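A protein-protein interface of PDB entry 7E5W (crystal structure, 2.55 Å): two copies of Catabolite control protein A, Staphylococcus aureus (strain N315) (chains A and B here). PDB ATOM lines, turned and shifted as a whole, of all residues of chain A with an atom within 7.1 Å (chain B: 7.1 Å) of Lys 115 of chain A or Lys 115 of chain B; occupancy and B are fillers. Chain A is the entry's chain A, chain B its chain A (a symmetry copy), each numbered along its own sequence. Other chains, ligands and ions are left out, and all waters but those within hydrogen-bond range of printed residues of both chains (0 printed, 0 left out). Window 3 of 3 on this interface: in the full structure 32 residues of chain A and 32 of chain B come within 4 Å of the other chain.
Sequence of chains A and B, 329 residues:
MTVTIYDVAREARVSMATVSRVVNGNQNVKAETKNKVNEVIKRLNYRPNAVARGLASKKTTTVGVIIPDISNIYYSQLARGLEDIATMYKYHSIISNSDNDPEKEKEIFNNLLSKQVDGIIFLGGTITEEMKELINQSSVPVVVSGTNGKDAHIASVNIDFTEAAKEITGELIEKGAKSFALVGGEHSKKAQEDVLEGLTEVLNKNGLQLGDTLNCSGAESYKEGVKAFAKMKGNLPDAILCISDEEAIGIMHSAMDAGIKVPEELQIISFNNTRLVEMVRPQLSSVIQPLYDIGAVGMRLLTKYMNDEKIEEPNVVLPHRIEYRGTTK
Among the printed residues, pairs that only touch across the chains: His 92 of chain A with Asn 111 of chain B (3.4 Å), Ile 94 of chain A with Ile 94 of chain B (3.9 Å), Asn 111 of chain A with His 92 of chain B (3.4 Å) and Lys 115 of chain A with Lys 115 of chain B (3.1 Å).
The side-chain hydroxyl (OG1) of Thr 62 of chain A is in hydrogen-bond range of the side-chain amide oxygen (OD1) of Asn 111 of chain B. OG1 of Thr 62 of chain A is in hydrogen-bond range of NZ of Lys 115 of chain B, at 2.7 Å. OD1 of Asn 111 of chain A sits at hydrogen-bond distance from OG1 of Thr 62 of chain B. The side-chain hydroxyl (OG1) of Thr 62 of chain B is in hydrogen-bond range of the side-chain amino group (NZ) of Lys 115 of chain A (2.7 Å).
Of chain B, only Thr 62 and Lys 115 come within 4 Å of Lys 115 of chain A. Of chain A, only Thr 62 and Lys 115 come within 4 Å of Lys 115 of chain B. Of the printed residues of chain A, Asn 111 of chain B touches Thr 62 and His 92. Of the printed residues of chain A, Ile 94 of chain B touches Ile 94. Of the printed residues of chain B, Asn 111 of chain A touches Thr 62 and His 92. Asn 110 of chain A touches none of the printed residues of chain B. The nearest residue of chain B that does not touch Lys 115 of chain A is Gln 116 of chain B (4.4 Å).
OD2 of Asp 118 of chain A sits at hydrogen-bond distance from N of Thr 62 of chain A (2.9 Å). The backbone NH (N) of Ile 94 of chain A is in hydrogen-bond range of the backbone carbonyl oxygen (O) of Val 63 of chain A, 2.9 Å away. The backbone carbonyl oxygen of Asn 111 of chain A lies within hydrogen-bond range of the side-chain hydroxyl of Ser 114 of chain A. The side-chain amino group (NZ) of Lys 115 of chain A is in hydrogen-bond range of the side-chain amide oxygen (OD1) of Asn 111 of chain A (3.2 Å). The backbone carbonyl oxygen (O) of Val 63 of chain B sits at hydrogen-bond distance from the backbone NH (N) of Ile 94 of chain B (2.9 Å). OD1 of Asn 111 of chain B is in hydrogen-bond range of NZ of Lys 115 of chain B, 3.2 Å away.
Of the 16 printed residues of chain B, 5 touch a printed residue of chain A. Printed residues of chain B that touch a printed residue of chain A: Thr 62, His 92, Ile 94, Asn 111 and Lys 115. Hydrophobic or aromatic side chains of chain A that line the printed part of chain B: His 92 and Ile 94.
Thr 62 of chain A touches Asn 111 of chain B, and with the chains exchanged Asn 111 of chain A touches Thr 62 of chain B. Thr 62 of chain A touches Lys 115 of chain B, and with the chains exchanged Lys 115 of chain A touches Thr 62 of chain B. His 92 of chain A touches Asn 111 of chain B, and with the chains exchanged Asn 111 of chain A touches His 92 of chain B. Lys 115 of chain A touches its own counterpart, Lys 115 of chain B. Of the 8 pairs that touch across the chains among the printed residues, 8 have their exchanged pair printed and touching as well.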
ATOM      1  N   THR A  60       4.527  28.420 -15.291  1.00  0.00           N
ATOM      2  CA  THR A  60       4.148  29.010 -14.011  1.00  0.00           C
ATOM      3  C   THR A  60       5.298  28.847 -13.023  1.00  0.00           C
ATOM      4  O   THR A  60       5.930  27.791 -12.962  1.00  0.00           O
ATOM      5  CB  THR A  60       2.881  28.361 -13.455  1.00  0.00           C
ATOM      6  OG1 THR A  60       2.660  28.800 -12.104  1.00  0.00           O
ATOM      7  CG2 THR A  60       3.022  26.855 -13.473  1.00  0.00           C
ATOM      8  N   THR A  61       5.585  29.901 -12.256  1.00  0.00           N
ATOM      9  CA  THR A  61       6.803  29.942 -11.456  1.00  0.00           C
ATOM     10  C   THR A  61       6.481  30.339 -10.026  1.00  0.00           C
ATOM     11  O   THR A  61       5.755  31.314  -9.791  1.00  0.00           O
ATOM     12  CB  THR A  61       7.837  30.911 -12.051  1.00  0.00           C
ATOM     13  OG1 THR A  61       8.131  30.528 -13.400  1.00  0.00           O
ATOM     14  CG2 THR A  61       9.128  30.910 -11.230  1.00  0.00           C
ATOM     15  N   THR A  62       7.034  29.584  -9.078  1.00  0.00           N
ATOM     16  CA  THR A  62       6.852  29.829  -7.655  1.00  0.00           C
ATOM     17  C   THR A  62       8.226  29.954  -7.010  1.00  0.00           C
ATOM     18  O   THR A  62       9.064  29.053  -7.135  1.00  0.00           O
ATOM     19  CB  THR A  62       6.057  28.704  -7.004  1.00  0.00           C
ATOM     20  OG1 THR A  62       4.793  28.589  -7.658  1.00  0.00           O
ATOM     21  CG2 THR A  62       5.834  28.973  -5.522  1.00  0.00           C
ATOM     22  N   VAL A  63       8.458  31.073  -6.344  1.00  0.00           N
ATOM     23  CA  VAL A  63       9.672  31.298  -5.582  1.00  0.00           C
ATOM     24  C   VAL A  63       9.357  31.073  -4.106  1.00  0.00           C
ATOM     25  O   VAL A  63       8.378  31.626  -3.575  1.00  0.00           O
ATOM     26  CB  VAL A  63      10.216  32.713  -5.832  1.00  0.00           C
ATOM     27  CG1 VAL A  63      11.522  32.940  -5.066  1.00  0.00           C
ATOM     28  CG2 VAL A  63      10.380  32.955  -7.330  1.00  0.00           C
ATOM     29  N   HIS A  92       4.585  33.513  -8.657  1.00  0.00           N
ATOM     30  CA  HIS A  92       4.039  33.277  -7.335  1.00  0.00           C
ATOM     31  C   HIS A  92       5.183  33.168  -6.327  1.00  0.00           C
ATOM     32  O   HIS A  92       6.341  32.928  -6.683  1.00  0.00           O
ATOM     33  CB  HIS A  92       3.186  32.010  -7.342  1.00  0.00           C
ATOM     34  CG  HIS A  92       2.226  31.956  -8.489  1.00  0.00           C
ATOM     35  ND1 HIS A  92       1.146  32.813  -8.600  1.00  0.00           N
ATOM     36  CD2 HIS A  92       2.201  31.172  -9.591  1.00  0.00           C
ATOM     37  CE1 HIS A  92       0.492  32.548  -9.715  1.00  0.00           C
ATOM     38  NE2 HIS A  92       1.108  31.554 -10.334  1.00  0.00           N
ATOM     39  N   ILE A  94       5.998  32.078  -1.926  1.00  0.00           N
ATOM     40  CA  ILE A  94       5.541  31.544  -0.654  1.00  0.00           C
ATOM     41  C   ILE A  94       6.684  31.647   0.349  1.00  0.00           C
ATOM     42  O   ILE A  94       7.840  31.339   0.025  1.00  0.00           O
ATOM     43  CB  ILE A  94       5.033  30.102  -0.822  1.00  0.00           C
ATOM     44  CG1 ILE A  94       6.049  29.246  -1.569  1.00  0.00           C
ATOM     45  CG2 ILE A  94       3.710  30.095  -1.614  1.00  0.00           C
ATOM     46  CD1 ILE A  94       5.594  27.751  -1.715  1.00  0.00           C
ATOM     47  N   PHE A 109      12.968  23.479   3.520  1.00  0.00           N
ATOM     48  CA  PHE A 109      13.590  23.205   2.227  1.00  0.00           C
ATOM     49  C   PHE A 109      12.936  22.011   1.550  1.00  0.00           C
ATOM     50  O   PHE A 109      12.503  22.090   0.400  1.00  0.00           O
ATOM     51  CB  PHE A 109      15.084  22.963   2.431  1.00  0.00           C
ATOM     52  CG  PHE A 109      15.890  22.935   1.164  1.00  0.00           C
ATOM     53  CD1 PHE A 109      16.203  24.114   0.493  1.00  0.00           C
ATOM     54  CD2 PHE A 109      16.371  21.740   0.664  1.00  0.00           C
ATOM     55  CE1 PHE A 109      16.969  24.097  -0.669  1.00  0.00           C
ATOM     56  CE2 PHE A 109      17.126  21.708  -0.507  1.00  0.00           C
ATOM     57  CZ  PHE A 109      17.436  22.891  -1.171  1.00  0.00           C
ATOM     58  N   ASN A 110      12.812  20.900   2.268  1.00  0.00           N
ATOM     59  CA  ASN A 110      12.271  19.708   1.635  1.00  0.00           C
ATOM     60  C   ASN A 110      10.789  19.878   1.312  1.00  0.00           C
ATOM     61  O   ASN A 110      10.309  19.331   0.311  1.00  0.00           O
ATOM     62  CB  ASN A 110      12.529  18.499   2.530  1.00  0.00           C
ATOM     63  CG  ASN A 110      13.995  18.066   2.507  1.00  0.00           C
ATOM     64  OD1 ASN A 110      14.666  18.172   1.481  1.00  0.00           O
ATOM     65  ND2 ASN A 110      14.501  17.604   3.645  1.00  0.00           N
ATOM     66  N   ASN A 111      10.060  20.648   2.124  1.00  0.00           N
ATOM     67  CA  ASN A 111       8.668  20.940   1.802  1.00  0.00           C
ATOM     68  C   ASN A 111       8.566  21.748   0.532  1.00  0.00           C
ATOM     69  O   ASN A 111       7.713  21.466  -0.322  1.00  0.00           O
ATOM     70  CB  ASN A 111       7.982  21.690   2.935  1.00  0.00           C
ATOM     71  CG  ASN A 111       6.476  21.817   2.714  1.00  0.00           C
ATOM     72  OD1 ASN A 111       5.794  20.832   2.431  1.00  0.00           O
ATOM     73  ND2 ASN A 111       5.957  23.030   2.848  1.00  0.00           N
ATOM     74  N   LEU A 112       9.418  22.765   0.383  1.00  0.00           N
ATOM     75  CA  LEU A 112       9.346  23.596  -0.817  1.00  0.00           C
ATOM     76  C   LEU A 112       9.715  22.780  -2.052  1.00  0.00           C
ATOM     77  O   LEU A 112       9.091  22.923  -3.109  1.00  0.00           O
ATOM     78  CB  LEU A 112      10.254  24.825  -0.682  1.00  0.00           C
ATOM     79  CG  LEU A 112      10.049  25.866   0.434  1.00  0.00           C
ATOM     80  CD1 LEU A 112      11.101  26.984   0.323  1.00  0.00           C
ATOM     81  CD2 LEU A 112       8.658  26.454   0.432  1.00  0.00           C
ATOM     82  N   LEU A 113      10.708  21.892  -1.932  1.00  0.00           N
ATOM     83  CA  LEU A 113      11.087  21.064  -3.071  1.00  0.00           C
ATOM     84  C   LEU A 113       9.944  20.136  -3.465  1.00  0.00           C
ATOM     85  O   LEU A 113       9.618  20.004  -4.651  1.00  0.00           O
ATOM     86  CB  LEU A 113      12.360  20.260  -2.762  1.00  0.00           C
ATOM     87  CG  LEU A 113      13.745  20.930  -2.595  1.00  0.00           C
ATOM     88  CD1 LEU A 113      14.880  19.895  -2.665  1.00  0.00           C
ATOM     89  CD2 LEU A 113      13.998  22.060  -3.588  1.00  0.00           C
ATOM     90  N   SER A 114       9.304  19.497  -2.478  1.00  0.00           N
ATOM     91  CA  SER A 114       8.200  18.588  -2.782  1.00  0.00           C
ATOM     92  C   SER A 114       7.007  19.322  -3.383  1.00  0.00           C
ATOM     93  O   SER A 114       6.237  18.725  -4.143  1.00  0.00           O
ATOM     94  CB  SER A 114       7.773  17.825  -1.525  1.00  0.00           C
ATOM     95  OG  SER A 114       6.857  18.584  -0.758  1.00  0.00           O
ATOM     96  N   LYS A 115       6.814  20.599  -3.038  1.00  0.00           N
ATOM     97  CA  LYS A 115       5.801  21.417  -3.697  1.00  0.00           C
ATOM     98  C   LYS A 115       6.306  21.995  -5.016  1.00  0.00           C
ATOM     99  O   LYS A 115       5.592  22.789  -5.652  1.00  0.00           O
ATOM    100  CB  LYS A 115       5.330  22.552  -2.770  1.00  0.00           C
ATOM    101  CG  LYS A 115       4.644  22.095  -1.490  1.00  0.00           C
ATOM    102  CD  LYS A 115       3.661  20.970  -1.756  1.00  0.00           C
ATOM    103  CE  LYS A 115       2.713  20.765  -0.589  1.00  0.00           C
ATOM    104  NZ  LYS A 115       3.251  21.454   0.628  1.00  0.00           N
ATOM    105  N   GLN A 116       7.528  21.642  -5.415  1.00  0.00           N
ATOM    106  CA  GLN A 116       8.037  21.932  -6.750  1.00  0.00           C
ATOM    107  C   GLN A 116       8.169  23.434  -7.015  1.00  0.00           C
ATOM    108  O   GLN A 116       7.816  23.930  -8.079  1.00  0.00           O
ATOM    109  CB  GLN A 116       7.167  21.242  -7.807  1.00  0.00           C
ATOM    110  CG  GLN A 116       7.380  19.724  -7.785  1.00  0.00           C
ATOM    111  CD  GLN A 116       6.438  18.951  -8.674  1.00  0.00           C
ATOM    112  OE1 GLN A 116       5.293  19.345  -8.871  1.00  0.00           O
ATOM    113  NE2 GLN A 116       6.920  17.836  -9.219  1.00  0.00           N
ATOM    114  N   VAL A 117       8.738  24.154  -6.047  1.00  0.00           N
ATOM    115  CA  VAL A 117       9.149  25.530  -6.299  1.00  0.00           C
ATOM    116  C   VAL A 117      10.313  25.548  -7.286  1.00  0.00           C
ATOM    117  O   VAL A 117      11.091  24.588  -7.395  1.00  0.00           O
ATOM    118  CB  VAL A 117       9.529  26.248  -4.990  1.00  0.00           C
ATOM    119  CG1 VAL A 117       8.436  26.089  -3.967  1.00  0.00           C
ATOM    120  CG2 VAL A 117      10.838  25.722  -4.456  1.00  0.00           C
ATOM    121  N   ASP A 118      10.446  26.658  -8.008  1.00  0.00           N
ATOM    122  CA  ASP A 118      11.430  26.773  -9.075  1.00  0.00           C
ATOM    123  C   ASP A 118      12.691  27.498  -8.649  1.00  0.00           C
ATOM    124  O   ASP A 118      13.637  27.588  -9.435  1.00  0.00           O
ATOM    125  CB  ASP A 118      10.811  27.504 -10.268  1.00  0.00           C
ATOM    126  CG  ASP A 118       9.510  26.885 -10.703  1.00  0.00           C
ATOM    127  OD1 ASP A 118       9.569  25.806 -11.317  1.00  0.00           O
ATOM    128  OD2 ASP A 118       8.435  27.463 -10.427  1.00  0.00           O
ATOM    129  N   THR B  60       1.390  14.177   5.574  1.00  0.00           N
ATOM    130  CA  THR B  60       2.097  15.454   5.617  1.00  0.00           C
ATOM    131  C   THR B  60       1.117  16.581   5.313  1.00  0.00           C
ATOM    132  O   THR B  60       0.279  16.462   4.418  1.00  0.00           O
ATOM    133  CB  THR B  60       3.255  15.479   4.620  1.00  0.00           C
ATOM    134  OG1 THR B  60       3.787  16.811   4.524  1.00  0.00           O
ATOM    135  CG2 THR B  60       2.772  15.037   3.256  1.00  0.00           C
ATOM    136  N   THR B  61       1.208  17.676   6.070  1.00  0.00           N
ATOM    137  CA  THR B  61       0.178  18.708   6.031  1.00  0.00           C
ATOM    138  C   THR B  61       0.811  20.077   5.853  1.00  0.00           C
ATOM    139  O   THR B  61       1.769  20.424   6.555  1.00  0.00           O
ATOM    140  CB  THR B  61      -0.688  18.690   7.299  1.00  0.00           C
ATOM    141  OG1 THR B  61      -1.277  17.393   7.458  1.00  0.00           O
ATOM    142  CG2 THR B  61      -1.795  19.745   7.225  1.00  0.00           C
ATOM    143  N   THR B  62       0.261  20.851   4.918  1.00  0.00           N
ATOM    144  CA  THR B  62       0.723  22.199   4.625  1.00  0.00           C
ATOM    145  C   THR B  62      -0.461  23.149   4.742  1.00  0.00           C
ATOM    146  O   THR B  62      -1.493  22.952   4.088  1.00  0.00           O
ATOM    147  CB  THR B  62       1.334  22.277   3.231  1.00  0.00           C
ATOM    148  OG1 THR B  62       2.415  21.348   3.145  1.00  0.00           O
ATOM    149  CG2 THR B  62       1.850  23.678   2.933  1.00  0.00           C
ATOM    150  N   VAL B  63      -0.319  24.158   5.585  1.00  0.00           N
ATOM    151  CA  VAL B  63      -1.309  25.209   5.727  1.00  0.00           C
ATOM    152  C   VAL B  63      -0.818  26.434   4.961  1.00  0.00           C
ATOM    153  O   VAL B  63       0.334  26.868   5.130  1.00  0.00           O
ATOM    154  CB  VAL B  63      -1.548  25.534   7.211  1.00  0.00           C
ATOM    155  CG1 VAL B  63      -2.624  26.610   7.369  1.00  0.00           C
ATOM    156  CG2 VAL B  63      -1.893  24.259   7.977  1.00  0.00           C
ATOM    157  N   HIS B  92       3.581  21.873   8.008  1.00  0.00           N
ATOM    158  CA  HIS B  92       4.265  22.899   7.246  1.00  0.00           C
ATOM    159  C   HIS B  92       3.307  24.060   6.983  1.00  0.00           C
ATOM    160  O   HIS B  92       2.083  23.923   7.073  1.00  0.00           O
ATOM    161  CB  HIS B  92       4.793  22.312   5.938  1.00  0.00           C
ATOM    162  CG  HIS B  92       5.515  21.014   6.127  1.00  0.00           C
ATOM    163  ND1 HIS B  92       6.730  20.925   6.781  1.00  0.00           N
ATOM    164  CD2 HIS B  92       5.180  19.751   5.777  1.00  0.00           C
ATOM    165  CE1 HIS B  92       7.115  19.663   6.815  1.00  0.00           C
ATOM    166  NE2 HIS B  92       6.196  18.930   6.209  1.00  0.00           N
ATOM    167  N   ILE B  94       2.990  27.985   4.593  1.00  0.00           N
ATOM    168  CA  ILE B  94       3.513  28.894   3.587  1.00  0.00           C
ATOM    169  C   ILE B  94       2.603  30.115   3.522  1.00  0.00           C
ATOM    170  O   ILE B  94       1.370  29.986   3.537  1.00  0.00           O
ATOM    171  CB  ILE B  94       3.643  28.183   2.228  1.00  0.00           C
ATOM    172  CG1 ILE B  94       2.350  27.465   1.859  1.00  0.00           C
ATOM    173  CG2 ILE B  94       4.782  27.145   2.279  1.00  0.00           C
ATOM    174  CD1 ILE B  94       2.420  26.771   0.453  1.00  0.00           C
ATOM    175  N   PHE B 109      -4.785  32.004  -4.100  1.00  0.00           N
ATOM    176  CA  PHE B 109      -5.655  30.868  -3.808  1.00  0.00           C
ATOM    177  C   PHE B 109      -5.411  29.729  -4.785  1.00  0.00           C
ATOM    178  O   PHE B 109      -5.165  28.590  -4.386  1.00  0.00           O
ATOM    179  CB  PHE B 109      -7.111  31.326  -3.858  1.00  0.00           C
ATOM    180  CG  PHE B 109      -8.098  30.330  -3.317  1.00  0.00           C
ATOM    181  CD1 PHE B 109      -8.236  30.140  -1.945  1.00  0.00           C
ATOM    182  CD2 PHE B 109      -8.914  29.615  -4.172  1.00  0.00           C
ATOM    183  CE1 PHE B 109      -9.164  29.236  -1.436  1.00  0.00           C
ATOM    184  CE2 PHE B 109      -9.836  28.695  -3.676  1.00  0.00           C
ATOM    185  CZ  PHE B 109      -9.971  28.512  -2.302  1.00  0.00           C
ATOM    186  N   ASN B 110      -5.430  30.026  -6.080  1.00  0.00           N
ATOM    187  CA  ASN B 110      -5.287  28.955  -7.052  1.00  0.00           C
ATOM    188  C   ASN B 110      -3.879  28.368  -7.024  1.00  0.00           C
ATOM    189  O   ASN B 110      -3.706  27.166  -7.263  1.00  0.00           O
ATOM    190  CB  ASN B 110      -5.667  29.474  -8.435  1.00  0.00           C
ATOM    191  CG  ASN B 110      -7.177  29.658  -8.590  1.00  0.00           C
ATOM    192  OD1 ASN B 110      -7.963  28.894  -8.029  1.00  0.00           O
ATOM    193  ND2 ASN B 110      -7.583  30.685  -9.326  1.00  0.00           N
ATOM    194  N   ASN B 111      -2.870  29.186  -6.710  1.00  0.00           N
ATOM    195  CA  ASN B 111      -1.520  28.657  -6.556  1.00  0.00           C
ATOM    196  C   ASN B 111      -1.444  27.706  -5.388  1.00  0.00           C
ATOM    197  O   ASN B 111      -0.829  26.635  -5.493  1.00  0.00           O
ATOM    198  CB  ASN B 111      -0.505  29.776  -6.364  1.00  0.00           C
ATOM    199  CG  ASN B 111       0.933  29.265  -6.415  1.00  0.00           C
ATOM    200  OD1 ASN B 111       1.315  28.547  -7.339  1.00  0.00           O
ATOM    201  ND2 ASN B 111       1.731  29.639  -5.424  1.00  0.00           N
ATOM    202  N   LEU B 112      -2.052  28.072  -4.258  1.00  0.00           N
ATOM    203  CA  LEU B 112      -1.988  27.199  -3.087  1.00  0.00           C
ATOM    204  C   LEU B 112      -2.729  25.893  -3.357  1.00  0.00           C
ATOM    205  O   LEU B 112      -2.270  24.817  -2.962  1.00  0.00           O
ATOM    206  CB  LEU B 112      -2.555  27.905  -1.850  1.00  0.00           C
ATOM    207  CG  LEU B 112      -1.939  29.207  -1.305  1.00  0.00           C
ATOM    208  CD1 LEU B 112      -2.710  29.686  -0.062  1.00  0.00           C
ATOM    209  CD2 LEU B 112      -0.468  29.065  -0.986  1.00  0.00           C
ATOM    210  N   LEU B 113      -3.866  25.962  -4.058  1.00  0.00           N
ATOM    211  CA  LEU B 113      -4.605  24.744  -4.370  1.00  0.00           C
ATOM    212  C   LEU B 113      -3.785  23.836  -5.278  1.00  0.00           C
ATOM    213  O   LEU B 113      -3.695  22.624  -5.045  1.00  0.00           O
ATOM    214  CB  LEU B 113      -5.962  25.077  -5.012  1.00  0.00           C
ATOM    215  CG  LEU B 113      -7.109  25.753  -4.226  1.00  0.00           C
ATOM    216  CD1 LEU B 113      -8.448  25.634  -4.974  1.00  0.00           C
ATOM    217  CD2 LEU B 113      -7.255  25.236  -2.798  1.00  0.00           C
ATOM    218  N   SER B 114      -3.157  24.406  -6.313  1.00  0.00           N
ATOM    219  CA  SER B 114      -2.356  23.596  -7.228  1.00  0.00           C
ATOM    220  C   SER B 114      -1.140  22.990  -6.536  1.00  0.00           C
ATOM    221  O   SER B 114      -0.662  21.930  -6.952  1.00  0.00           O
ATOM    222  CB  SER B 114      -1.917  24.428  -8.436  1.00  0.00           C
ATOM    223  OG  SER B 114      -0.739  25.159  -8.147  1.00  0.00           O
ATOM    224  N   LYS B 115      -0.606  23.653  -5.505  1.00  0.00           N
ATOM    225  CA  LYS B 115       0.446  23.061  -4.687  1.00  0.00           C
ATOM    226  C   LYS B 115      -0.119  22.133  -3.616  1.00  0.00           C
ATOM    227  O   LYS B 115       0.644  21.622  -2.779  1.00  0.00           O
ATOM    228  CB  LYS B 115       1.310  24.155  -4.033  1.00  0.00           C
ATOM    229  CG  LYS B 115       2.071  25.042  -5.009  1.00  0.00           C
ATOM    230  CD  LYS B 115       2.714  24.229  -6.116  1.00  0.00           C
ATOM    231  CE  LYS B 115       3.766  25.028  -6.862  1.00  0.00           C
ATOM    232  NZ  LYS B 115       3.605  26.486  -6.557  1.00  0.00           N
ATOM    233  N   GLN B 116      -1.438  21.936  -3.606  1.00  0.00           N
ATOM    234  CA  GLN B 116      -2.078  20.907  -2.796  1.00  0.00           C
ATOM    235  C   GLN B 116      -1.903  21.149  -1.294  1.00  0.00           C
ATOM    236  O   GLN B 116      -1.623  20.234  -0.527  1.00  0.00           O
ATOM    237  CB  GLN B 116      -1.572  19.521  -3.211  1.00  0.00           C
ATOM    238  CG  GLN B 116      -2.121  19.128  -4.588  1.00  0.00           C
ATOM    239  CD  GLN B 116      -1.539  17.855  -5.150  1.00  0.00           C
ATOM    240  OE1 GLN B 116      -0.382  17.530  -4.904  1.00  0.00           O
ATOM    241  NE2 GLN B 116      -2.346  17.122  -5.915  1.00  0.00           N
ATOM    242  N   VAL B 117      -2.127  22.393  -0.870  1.00  0.00           N
ATOM    243  CA  VAL B 117      -2.246  22.673   0.556  1.00  0.00           C
ATOM    244  C   VAL B 117      -3.520  22.032   1.102  1.00  0.00           C
ATOM    245  O   VAL B 117      -4.504  21.818   0.379  1.00  0.00           O
ATOM    246  CB  VAL B 117      -2.233  24.188   0.831  1.00  0.00           C
ATOM    247  CG1 VAL B 117      -1.054  24.836   0.154  1.00  0.00           C
ATOM    248  CG2 VAL B 117      -3.524  24.823   0.374  1.00  0.00           C
ATOM    249  N   ASP B 118      -3.510  21.733   2.399  1.00  0.00           N
ATOM    250  CA  ASP B 118      -4.601  21.007   3.033  1.00  0.00           C
ATOM    251  C   ASP B 118      -5.576  21.910   3.761  1.00  0.00           C
ATOM    252  O   ASP B 118      -6.591  21.428   4.269  1.00  0.00           O
ATOM    253  CB  ASP B 118      -4.034  19.984   4.019  1.00  0.00           C
ATOM    254  CG  ASP B 118      -2.998  19.096   3.384  1.00  0.00           C
ATOM    255  OD1 ASP B 118      -3.402  18.213   2.608  1.00  0.00           O
ATOM    256  OD2 ASP B 118      -1.789  19.280   3.650  1.00  0.00           O
